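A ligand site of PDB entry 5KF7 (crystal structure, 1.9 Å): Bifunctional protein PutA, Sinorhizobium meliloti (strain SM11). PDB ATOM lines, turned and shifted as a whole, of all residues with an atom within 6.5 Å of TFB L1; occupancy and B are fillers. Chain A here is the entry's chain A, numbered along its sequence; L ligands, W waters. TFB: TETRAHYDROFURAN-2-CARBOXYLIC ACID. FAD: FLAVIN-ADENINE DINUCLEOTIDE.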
ATOM      1  N   ASP A 223     -15.585 -12.083 -27.492  1.00  0.00           N
ATOM      2  CA  ASP A 223     -15.781 -10.987 -28.444  1.00  0.00           C
ATOM      3  C   ASP A 223     -15.630 -11.535 -29.855  1.00  0.00           C
ATOM      4  O   ASP A 223     -14.519 -11.891 -30.260  1.00  0.00           O
ATOM      5  CB  ASP A 223     -14.800  -9.851 -28.201  1.00  0.00           C
ATOM      6  CG  ASP A 223     -14.907  -8.780 -29.275  1.00  0.00           C
ATOM      7  OD1 ASP A 223     -16.038  -8.355 -29.582  1.00  0.00           O
ATOM      8  OD2 ASP A 223     -13.858  -8.397 -29.814  1.00  0.00           O
ATOM      9  N   GLU A 227     -16.061  -4.290 -35.680  1.00  0.00           N
ATOM     10  CA  GLU A 227     -16.241  -2.927 -35.216  1.00  0.00           C
ATOM     11  C   GLU A 227     -16.312  -2.036 -36.443  1.00  0.00           C
ATOM     12  O   GLU A 227     -15.930  -2.438 -37.540  1.00  0.00           O
ATOM     13  CB  GLU A 227     -15.088  -2.498 -34.302  1.00  0.00           C
ATOM     14  CG  GLU A 227     -13.766  -2.282 -35.015  1.00  0.00           C
ATOM     15  CD  GLU A 227     -12.599  -2.183 -34.061  1.00  0.00           C
ATOM     16  OE1 GLU A 227     -12.293  -3.177 -33.370  1.00  0.00           O
ATOM     17  OE2 GLU A 227     -11.984  -1.101 -33.972  1.00  0.00           O
ATOM     18  N   SER A 265     -19.252  -9.802 -25.130  1.00  0.00           N
ATOM     19  CA  SER A 265     -18.986  -8.379 -25.264  1.00  0.00           C
ATOM     20  C   SER A 265     -19.316  -7.971 -26.685  1.00  0.00           C
ATOM     21  O   SER A 265     -19.075  -8.727 -27.631  1.00  0.00           O
ATOM     22  CB  SER A 265     -17.516  -8.043 -24.935  1.00  0.00           C
ATOM     23  OG  SER A 265     -17.222  -8.273 -23.577  1.00  0.00           O
ATOM     24  N   LYS A 267     -19.535  -4.388 -29.521  1.00  0.00           N
ATOM     25  CA  LYS A 267     -19.219  -3.002 -29.836  1.00  0.00           C
ATOM     26  C   LYS A 267     -20.389  -2.414 -30.621  1.00  0.00           C
ATOM     27  O   LYS A 267     -20.831  -3.014 -31.608  1.00  0.00           O
ATOM     28  CB  LYS A 267     -17.924  -2.873 -30.642  1.00  0.00           C
ATOM     29  CG  LYS A 267     -16.649  -3.055 -29.811  1.00  0.00           C
ATOM     30  CD  LYS A 267     -15.404  -2.951 -30.714  1.00  0.00           C
ATOM     31  CE  LYS A 267     -14.101  -2.872 -29.916  1.00  0.00           C
ATOM     32  NZ  LYS A 267     -13.911  -4.027 -28.972  1.00  0.00           N
ATOM     33  N   ASN A 306     -21.928  -7.328 -22.381  1.00  0.00           N
ATOM     34  CA  ASN A 306     -21.174  -6.123 -22.076  1.00  0.00           C
ATOM     35  C   ASN A 306     -21.039  -5.252 -23.320  1.00  0.00           C
ATOM     36  O   ASN A 306     -20.674  -5.736 -24.383  1.00  0.00           O
ATOM     37  CB  ASN A 306     -19.781  -6.469 -21.536  1.00  0.00           C
ATOM     38  CG  ASN A 306     -18.916  -5.245 -21.339  1.00  0.00           C
ATOM     39  OD1 ASN A 306     -18.973  -4.577 -20.294  1.00  0.00           O
ATOM     40  ND2 ASN A 306     -18.134  -4.909 -22.362  1.00  0.00           N
ATOM     41  N   ASP A 308     -18.810  -2.662 -25.010  1.00  0.00           N
ATOM     42  CA  ASP A 308     -17.468  -2.087 -24.996  1.00  0.00           C
ATOM     43  C   ASP A 308     -17.529  -0.585 -25.178  1.00  0.00           C
ATOM     44  O   ASP A 308     -18.446  -0.041 -25.809  1.00  0.00           O
ATOM     45  CB  ASP A 308     -16.594  -2.705 -26.099  1.00  0.00           C
ATOM     46  CG  ASP A 308     -16.227  -4.176 -25.839  1.00  0.00           C
ATOM     47  OD1 ASP A 308     -16.406  -4.662 -24.689  1.00  0.00           O
ATOM     48  OD2 ASP A 308     -15.772  -4.845 -26.783  1.00  0.00           O
ATOM     49  N   ALA A 309     -16.545   0.108 -24.609  1.00  0.00           N
ATOM     50  CA  ALA A 309     -16.415   1.551 -24.780  1.00  0.00           C
ATOM     51  C   ALA A 309     -15.479   1.834 -25.937  1.00  0.00           C
ATOM     52  O   ALA A 309     -14.470   1.132 -26.141  1.00  0.00           O
ATOM     53  CB  ALA A 309     -15.913   2.211 -23.494  1.00  0.00           C
ATOM     54  N   VAL A 340     -18.734  -0.697 -20.131  1.00  0.00           N
ATOM     55  CA  VAL A 340     -17.349  -0.314 -19.864  1.00  0.00           C
ATOM     56  C   VAL A 340     -17.291   1.179 -19.600  1.00  0.00           C
ATOM     57  O   VAL A 340     -17.952   1.966 -20.284  1.00  0.00           O
ATOM     58  CB  VAL A 340     -16.457  -0.691 -21.058  1.00  0.00           C
ATOM     59  CG1 VAL A 340     -15.023  -0.196 -20.838  1.00  0.00           C
ATOM     60  CG2 VAL A 340     -16.498  -2.190 -21.298  1.00  0.00           C
ATOM     61  N   ARG A 369     -17.451  -2.647 -16.221  1.00  0.00           N
ATOM     62  CA  ARG A 369     -16.056  -2.976 -16.469  1.00  0.00           C
ATOM     63  C   ARG A 369     -15.242  -1.697 -16.424  1.00  0.00           C
ATOM     64  O   ARG A 369     -15.399  -0.829 -17.293  1.00  0.00           O
ATOM     65  CB  ARG A 369     -15.882  -3.676 -17.817  1.00  0.00           C
ATOM     66  CG  ARG A 369     -14.419  -4.098 -18.071  1.00  0.00           C
ATOM     67  CD  ARG A 369     -14.170  -4.441 -19.537  1.00  0.00           C
ATOM     68  NE  ARG A 369     -14.864  -5.659 -19.958  1.00  0.00           N
ATOM     69  CZ  ARG A 369     -15.154  -5.947 -21.218  1.00  0.00           C
ATOM     70  NH1 ARG A 369     -14.804  -5.104 -22.196  1.00  0.00           N
ATOM     71  NH2 ARG A 369     -15.789  -7.066 -21.519  1.00  0.00           N
ATOM     72  N   ALA A 374      -8.349   2.278 -24.607  1.00  0.00           N
ATOM     73  CA  ALA A 374      -7.601   1.685 -25.729  1.00  0.00           C
ATOM     74  C   ALA A 374      -7.348   2.632 -26.888  1.00  0.00           C
ATOM     75  O   ALA A 374      -6.729   2.218 -27.877  1.00  0.00           O
ATOM     76  CB  ALA A 374      -8.319   0.425 -26.240  1.00  0.00           C
ATOM     77  N   TYR A 375      -7.787   3.900 -26.824  1.00  0.00           N
ATOM     78  CA  TYR A 375      -7.780   4.796 -27.979  1.00  0.00           C
ATOM     79  C   TYR A 375      -6.961   6.062 -27.722  1.00  0.00           C
ATOM     80  O   TYR A 375      -7.199   7.092 -28.353  1.00  0.00           O
ATOM     81  CB  TYR A 375      -9.226   5.151 -28.380  1.00  0.00           C
ATOM     82  CG  TYR A 375     -10.081   3.935 -28.657  1.00  0.00           C
ATOM     83  CD1 TYR A 375     -10.768   3.282 -27.633  1.00  0.00           C
ATOM     84  CD2 TYR A 375     -10.196   3.416 -29.944  1.00  0.00           C
ATOM     85  CE1 TYR A 375     -11.528   2.149 -27.882  1.00  0.00           C
ATOM     86  CE2 TYR A 375     -10.963   2.290 -30.207  1.00  0.00           C
ATOM     87  CZ  TYR A 375     -11.633   1.660 -29.171  1.00  0.00           C
ATOM     88  OH  TYR A 375     -12.387   0.540 -29.436  1.00  0.00           O
ATOM     89  N   LEU A 451      -7.148  -9.606 -20.729  1.00  0.00           N
ATOM     90  CA  LEU A 451      -7.265  -9.928 -22.142  1.00  0.00           C
ATOM     91  C   LEU A 451      -6.550 -11.233 -22.446  1.00  0.00           C
ATOM     92  O   LEU A 451      -5.474 -11.512 -21.896  1.00  0.00           O
ATOM     93  CB  LEU A 451      -6.694  -8.793 -23.007  1.00  0.00           C
ATOM     94  CG  LEU A 451      -7.329  -7.429 -22.795  1.00  0.00           C
ATOM     95  CD1 LEU A 451      -6.469  -6.320 -23.383  1.00  0.00           C
ATOM     96  CD2 LEU A 451      -8.745  -7.389 -23.379  1.00  0.00           C
ATOM     97  N   TYR A 475     -11.236 -11.724 -21.399  1.00  0.00           N
ATOM     98  CA  TYR A 475     -11.810 -11.224 -22.637  1.00  0.00           C
ATOM     99  C   TYR A 475     -11.185 -11.999 -23.800  1.00  0.00           C
ATOM    100  O   TYR A 475      -9.972 -11.938 -24.001  1.00  0.00           O
ATOM    101  CB  TYR A 475     -11.521  -9.724 -22.760  1.00  0.00           C
ATOM    102  CG  TYR A 475     -12.217  -9.001 -23.893  1.00  0.00           C
ATOM    103  CD1 TYR A 475     -11.667  -8.974 -25.184  1.00  0.00           C
ATOM    104  CD2 TYR A 475     -13.406  -8.304 -23.683  1.00  0.00           C
ATOM    105  CE1 TYR A 475     -12.291  -8.293 -26.225  1.00  0.00           C
ATOM    106  CE2 TYR A 475     -14.029  -7.620 -24.715  1.00  0.00           C
ATOM    107  CZ  TYR A 475     -13.481  -7.623 -25.972  1.00  0.00           C
ATOM    108  OH  TYR A 475     -14.120  -6.949 -26.988  1.00  0.00           O
ATOM    109  N   ALA A 486      -7.580  -4.555 -36.575  1.00  0.00           N
ATOM    110  CA  ALA A 486      -7.679  -3.380 -35.708  1.00  0.00           C
ATOM    111  C   ALA A 486      -7.434  -3.743 -34.250  1.00  0.00           C
ATOM    112  O   ALA A 486      -6.636  -3.105 -33.557  1.00  0.00           O
ATOM    113  CB  ALA A 486      -9.047  -2.716 -35.882  1.00  0.00           C
ATOM    114  N   TYR A 487      -8.107  -4.789 -33.767  1.00  0.00           N
ATOM    115  CA  TYR A 487      -7.949  -5.220 -32.376  1.00  0.00           C
ATOM    116  C   TYR A 487      -6.529  -5.710 -32.102  1.00  0.00           C
ATOM    117  O   TYR A 487      -5.980  -5.458 -31.016  1.00  0.00           O
ATOM    118  CB  TYR A 487      -8.967  -6.321 -32.058  1.00  0.00           C
ATOM    119  CG  TYR A 487      -8.804  -6.960 -30.700  1.00  0.00           C
ATOM    120  CD1 TYR A 487      -7.893  -7.990 -30.494  1.00  0.00           C
ATOM    121  CD2 TYR A 487      -9.605  -6.563 -29.625  1.00  0.00           C
ATOM    122  CE1 TYR A 487      -7.749  -8.592 -29.248  1.00  0.00           C
ATOM    123  CE2 TYR A 487      -9.470  -7.161 -28.381  1.00  0.00           C
ATOM    124  CZ  TYR A 487      -8.551  -8.168 -28.195  1.00  0.00           C
ATOM    125  OH  TYR A 487      -8.435  -8.761 -26.952  1.00  0.00           O
ATOM    126  N   ARG A 490      -4.074  -2.804 -31.631  1.00  0.00           N
ATOM    127  CA  ARG A 490      -4.264  -2.175 -30.329  1.00  0.00           C
ATOM    128  C   ARG A 490      -3.586  -2.970 -29.220  1.00  0.00           C
ATOM    129  O   ARG A 490      -2.920  -2.397 -28.356  1.00  0.00           O
ATOM    130  CB  ARG A 490      -5.758  -1.990 -30.041  1.00  0.00           C
ATOM    131  CG  ARG A 490      -6.416  -0.892 -30.876  1.00  0.00           C
ATOM    132  CD  ARG A 490      -7.744  -0.425 -30.275  1.00  0.00           C
ATOM    133  NE  ARG A 490      -8.756  -1.473 -30.283  1.00  0.00           N
ATOM    134  CZ  ARG A 490      -9.616  -1.685 -31.283  1.00  0.00           C
ATOM    135  NH1 ARG A 490      -9.581  -0.912 -32.355  1.00  0.00           N
ATOM    136  NH2 ARG A 490     -10.499  -2.661 -31.204  1.00  0.00           N
ATOM    137  N   ARG A 491      -3.735  -4.297 -29.248  1.00  0.00           N
ATOM    138  CA  ARG A 491      -3.035  -5.134 -28.273  1.00  0.00           C
ATOM    139  C   ARG A 491      -1.518  -4.975 -28.402  1.00  0.00           C
ATOM    140  O   ARG A 491      -0.816  -4.769 -27.408  1.00  0.00           O
ATOM    141  CB  ARG A 491      -3.436  -6.587 -28.449  1.00  0.00           C
ATOM    142  CG  ARG A 491      -4.922  -6.849 -28.299  1.00  0.00           C
ATOM    143  CD  ARG A 491      -5.388  -6.713 -26.850  1.00  0.00           C
ATOM    144  NE  ARG A 491      -5.470  -5.334 -26.374  1.00  0.00           N
ATOM    145  CZ  ARG A 491      -6.387  -4.456 -26.754  1.00  0.00           C
ATOM    146  NH1 ARG A 491      -7.307  -4.803 -27.664  1.00  0.00           N
ATOM    147  NH2 ARG A 491      -6.390  -3.231 -26.258  1.00  0.00           N
ATOM    148  N   GLU A 494      -0.308  -1.620 -27.172  1.00  0.00           N
ATOM    149  CA  GLU A 494      -0.345  -1.664 -25.723  1.00  0.00           C
ATOM    150  C   GLU A 494       0.807  -2.498 -25.159  1.00  0.00           C
ATOM    151  O   GLU A 494       1.407  -2.133 -24.142  1.00  0.00           O
ATOM    152  CB  GLU A 494      -1.698  -2.218 -25.269  1.00  0.00           C
ATOM    153  CG  GLU A 494      -1.794  -2.674 -23.819  1.00  0.00           C
ATOM    154  CD  GLU A 494      -3.140  -3.322 -23.499  1.00  0.00           C
ATOM    155  OE1 GLU A 494      -3.976  -3.496 -24.418  1.00  0.00           O
ATOM    156  OE2 GLU A 494      -3.354  -3.671 -22.320  1.00  0.00           O
HETATM  157  OA  TFB L   1     -12.249  -3.148 -26.110  1.00  0.00           O
HETATM  158  CA  TFB L   1     -10.848  -2.963 -26.161  1.00  0.00           C
HETATM  159  C   TFB L   1     -10.337  -3.081 -27.585  1.00  0.00           C
HETATM  160  OB  TFB L   1     -11.138  -3.426 -28.531  1.00  0.00           O
HETATM  161  CB  TFB L   1     -10.235  -4.009 -25.346  1.00  0.00           C
HETATM  162  CG  TFB L   1     -11.237  -5.056 -25.236  1.00  0.00           C
HETATM  163  CD  TFB L   1     -12.517  -4.424 -25.550  1.00  0.00           C
HETATM  164  OXT TFB L   1      -9.109  -2.843 -27.840  1.00  0.00           O
HETATM  165  PA  FAD L   2      -1.097  -0.009 -17.868  1.00  0.00           P
HETATM  166  O1A FAD L   2       0.326  -0.116 -18.459  1.00  0.00           O
HETATM  167  O2A FAD L   2      -1.233   0.240 -16.452  1.00  0.00           O
HETATM  168  O5B FAD L   2      -1.934   1.128 -18.380  1.00  0.00           O
HETATM  169  C5B FAD L   2      -1.867   1.478 -19.753  1.00  0.00           C
HETATM  170  C4B FAD L   2      -2.909   2.533 -20.140  1.00  0.00           C
HETATM  171  O4B FAD L   2      -2.573   3.824 -19.700  1.00  0.00           O
HETATM  172  C3B FAD L   2      -3.057   2.687 -21.611  1.00  0.00           C
HETATM  173  O3B FAD L   2      -3.812   1.698 -22.212  1.00  0.00           O
HETATM  174  C2B FAD L   2      -3.747   4.001 -21.723  1.00  0.00           C
HETATM  175  O2B FAD L   2      -5.097   3.849 -21.470  1.00  0.00           O
HETATM  176  C1B FAD L   2      -3.149   4.754 -20.597  1.00  0.00           C
HETATM  177  N9A FAD L   2      -2.153   5.718 -20.987  1.00  0.00           N
HETATM  178  C8A FAD L   2      -0.964   5.468 -21.644  1.00  0.00           C
HETATM  179  N7A FAD L   2      -0.284   6.605 -21.828  1.00  0.00           N
HETATM  180  C5A FAD L   2      -1.003   7.658 -21.289  1.00  0.00           C
HETATM  181  C6A FAD L   2      -0.797   9.028 -21.194  1.00  0.00           C
HETATM  182  N6A FAD L   2       0.409   9.630 -21.708  1.00  0.00           N
HETATM  183  N1A FAD L   2      -1.723   9.795 -20.585  1.00  0.00           N
HETATM  184  C2A FAD L   2      -2.856   9.261 -20.068  1.00  0.00           C
HETATM  185  N3A FAD L   2      -3.095   7.927 -20.156  1.00  0.00           N
HETATM  186  C4A FAD L   2      -2.215   7.112 -20.755  1.00  0.00           C
HETATM  187  N1  FAD L   2     -10.421  -0.153 -23.170  1.00  0.00           N
HETATM  188  C2  FAD L   2     -11.409   0.506 -23.989  1.00  0.00           C
HETATM  189  O2  FAD L   2     -11.114   1.726 -24.472  1.00  0.00           O
HETATM  190  N3  FAD L   2     -12.665  -0.066 -24.224  1.00  0.00           N
HETATM  191  C4  FAD L   2     -12.963  -1.321 -23.715  1.00  0.00           C
HETATM  192  O4  FAD L   2     -14.206  -1.858 -23.965  1.00  0.00           O
HETATM  193  C4X FAD L   2     -11.917  -2.090 -22.949  1.00  0.00           C
HETATM  194  N5  FAD L   2     -12.111  -3.394 -22.476  1.00  0.00           N
HETATM  195  C5X FAD L   2     -11.097  -4.042 -21.771  1.00  0.00           C
HETATM  196  C6  FAD L   2     -11.303  -5.356 -21.304  1.00  0.00           C
HETATM  197  C7  FAD L   2     -10.304  -6.015 -20.583  1.00  0.00           C
HETATM  198  C7M FAD L   2     -10.569  -7.412 -20.092  1.00  0.00           C
HETATM  199  C8  FAD L   2      -9.087  -5.390 -20.337  1.00  0.00           C
HETATM  200  C8M FAD L   2      -8.004  -6.105 -19.573  1.00  0.00           C
HETATM  201  C9  FAD L   2      -8.861  -4.082 -20.802  1.00  0.00           C
HETATM  202  C9A FAD L   2      -9.860  -3.419 -21.514  1.00  0.00           C
HETATM  203  N10 FAD L   2      -9.636  -2.085 -21.999  1.00  0.00           N
HETATM  204  C10 FAD L   2     -10.647  -1.429 -22.709  1.00  0.00           C
HETATM  205  C1' FAD L   2      -8.361  -1.393 -21.708  1.00  0.00           C
HETATM  206  C2' FAD L   2      -7.296  -1.361 -22.793  1.00  0.00           C
HETATM  207  O2' FAD L   2      -7.601  -2.191 -23.839  1.00  0.00           O
HETATM  208  C3' FAD L   2      -5.954  -1.731 -22.135  1.00  0.00           C
HETATM  209  O3' FAD L   2      -5.904  -3.087 -21.938  1.00  0.00           O
HETATM  210  C4' FAD L   2      -5.723  -1.052 -20.808  1.00  0.00           C
HETATM  211  O4' FAD L   2      -5.946   0.303 -20.958  1.00  0.00           O
HETATM  212  C5' FAD L   2      -4.339  -1.332 -20.199  1.00  0.00           C
HETATM  213  O5' FAD L   2      -4.302  -0.846 -18.863  1.00  0.00           O
HETATM  214  P   FAD L   2      -3.484  -1.562 -17.670  1.00  0.00           P
HETATM  215  O1P FAD L   2      -3.969  -1.335 -16.183  1.00  0.00           O
HETATM  216  O2P FAD L   2      -3.477  -3.018 -18.254  1.00  0.00           O
HETATM  217  O3P FAD L   2      -1.950  -1.231 -18.078  1.00  0.00           O
HETATM  218  O   HOH W   1     -13.340  -1.126 -27.312  1.00  0.00           O
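Water W1 lies within hydrogen-bond range of an oxygen (OA) of TFB L1 (2.6 Å), the backbone carbonyl oxygen of Ala 309 (2.8 Å), the side-chain hydroxyl of Tyr 375 (2.9 Å), a nitrogen (N3) of FAD L2 (3.3 Å) and the side-chain amino group of Lys 267 (3.4 Å).
An oxygen (OXT) of TFB L1 lies within salt-bridge range of the guanidinium group of Arg 491. OXT of TFB L1 is in salt-bridge range of NE of Arg 490 (2.8 Å). NZ of Lys 267 lies within salt-bridge range of OB of TFB L1 (2.9 Å). An oxygen (O2') of FAD L2 is in hydrogen-bond range of the guanidinium group (NH2) of Arg 491 (2.9 Å). The backbone NH of Ala 374 is in hydrogen-bond range of an oxygen (O2) of FAD L2 (2.8 Å). NH1 of Arg 369 sits at hydrogen-bond distance from N5 of FAD L2, 3.2 Å away. N of Ala 309 sits at hydrogen-bond distance from O4 of FAD L2, at 3.1 Å. O of Ala 309 is in hydrogen-bond range of N3 of FAD L2 (2.9 Å). The side-chain carboxylate (OE2) of Glu 494 lies within hydrogen-bond range of an oxygen (O3') of FAD L2 (2.6 Å).
Asp 308 touches TFB L1 (OD2 to CD, 3.5 Å). CB of Ala 374 touches OXT of TFB L1, at 3.7 Å. Leu 451 touches TFB L1. Tyr 475 touches TFB L1. Tyr 487 touches TFB L1. Hydrophobic or aromatic side chains that line TFB L1: Ala 374, Leu 451, Tyr 475 and Tyr 487. Of the 18 residues printed, 8 come within 4 Å of TFB L1.
The guanidinium group (NH2) of Arg 491 lies within salt-bridge range of the side-chain carboxylate (OE1) of Glu 494 (3.0 Å). The side-chain carboxylate of Glu 227 lies within salt-bridge range of the guanidinium group of Arg 490, 2.9 Å away. NZ of Lys 267 is in salt-bridge range of OD2 of Asp 308. OH of Tyr 475 is in hydrogen-bond range of OD2 of Asp 308 (2.7 Å). OD2 of Asp 223 lies close to OH of Tyr 475 (3.2 Å). The side-chain carboxylate (OD1) of Asp 308 is in salt-bridge range of the guanidinium group (NH1) of Arg 369 (3.0 Å). OD1 of Asp 308 is in hydrogen-bond range of ND2 of Asn 306 (2.9 Å).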
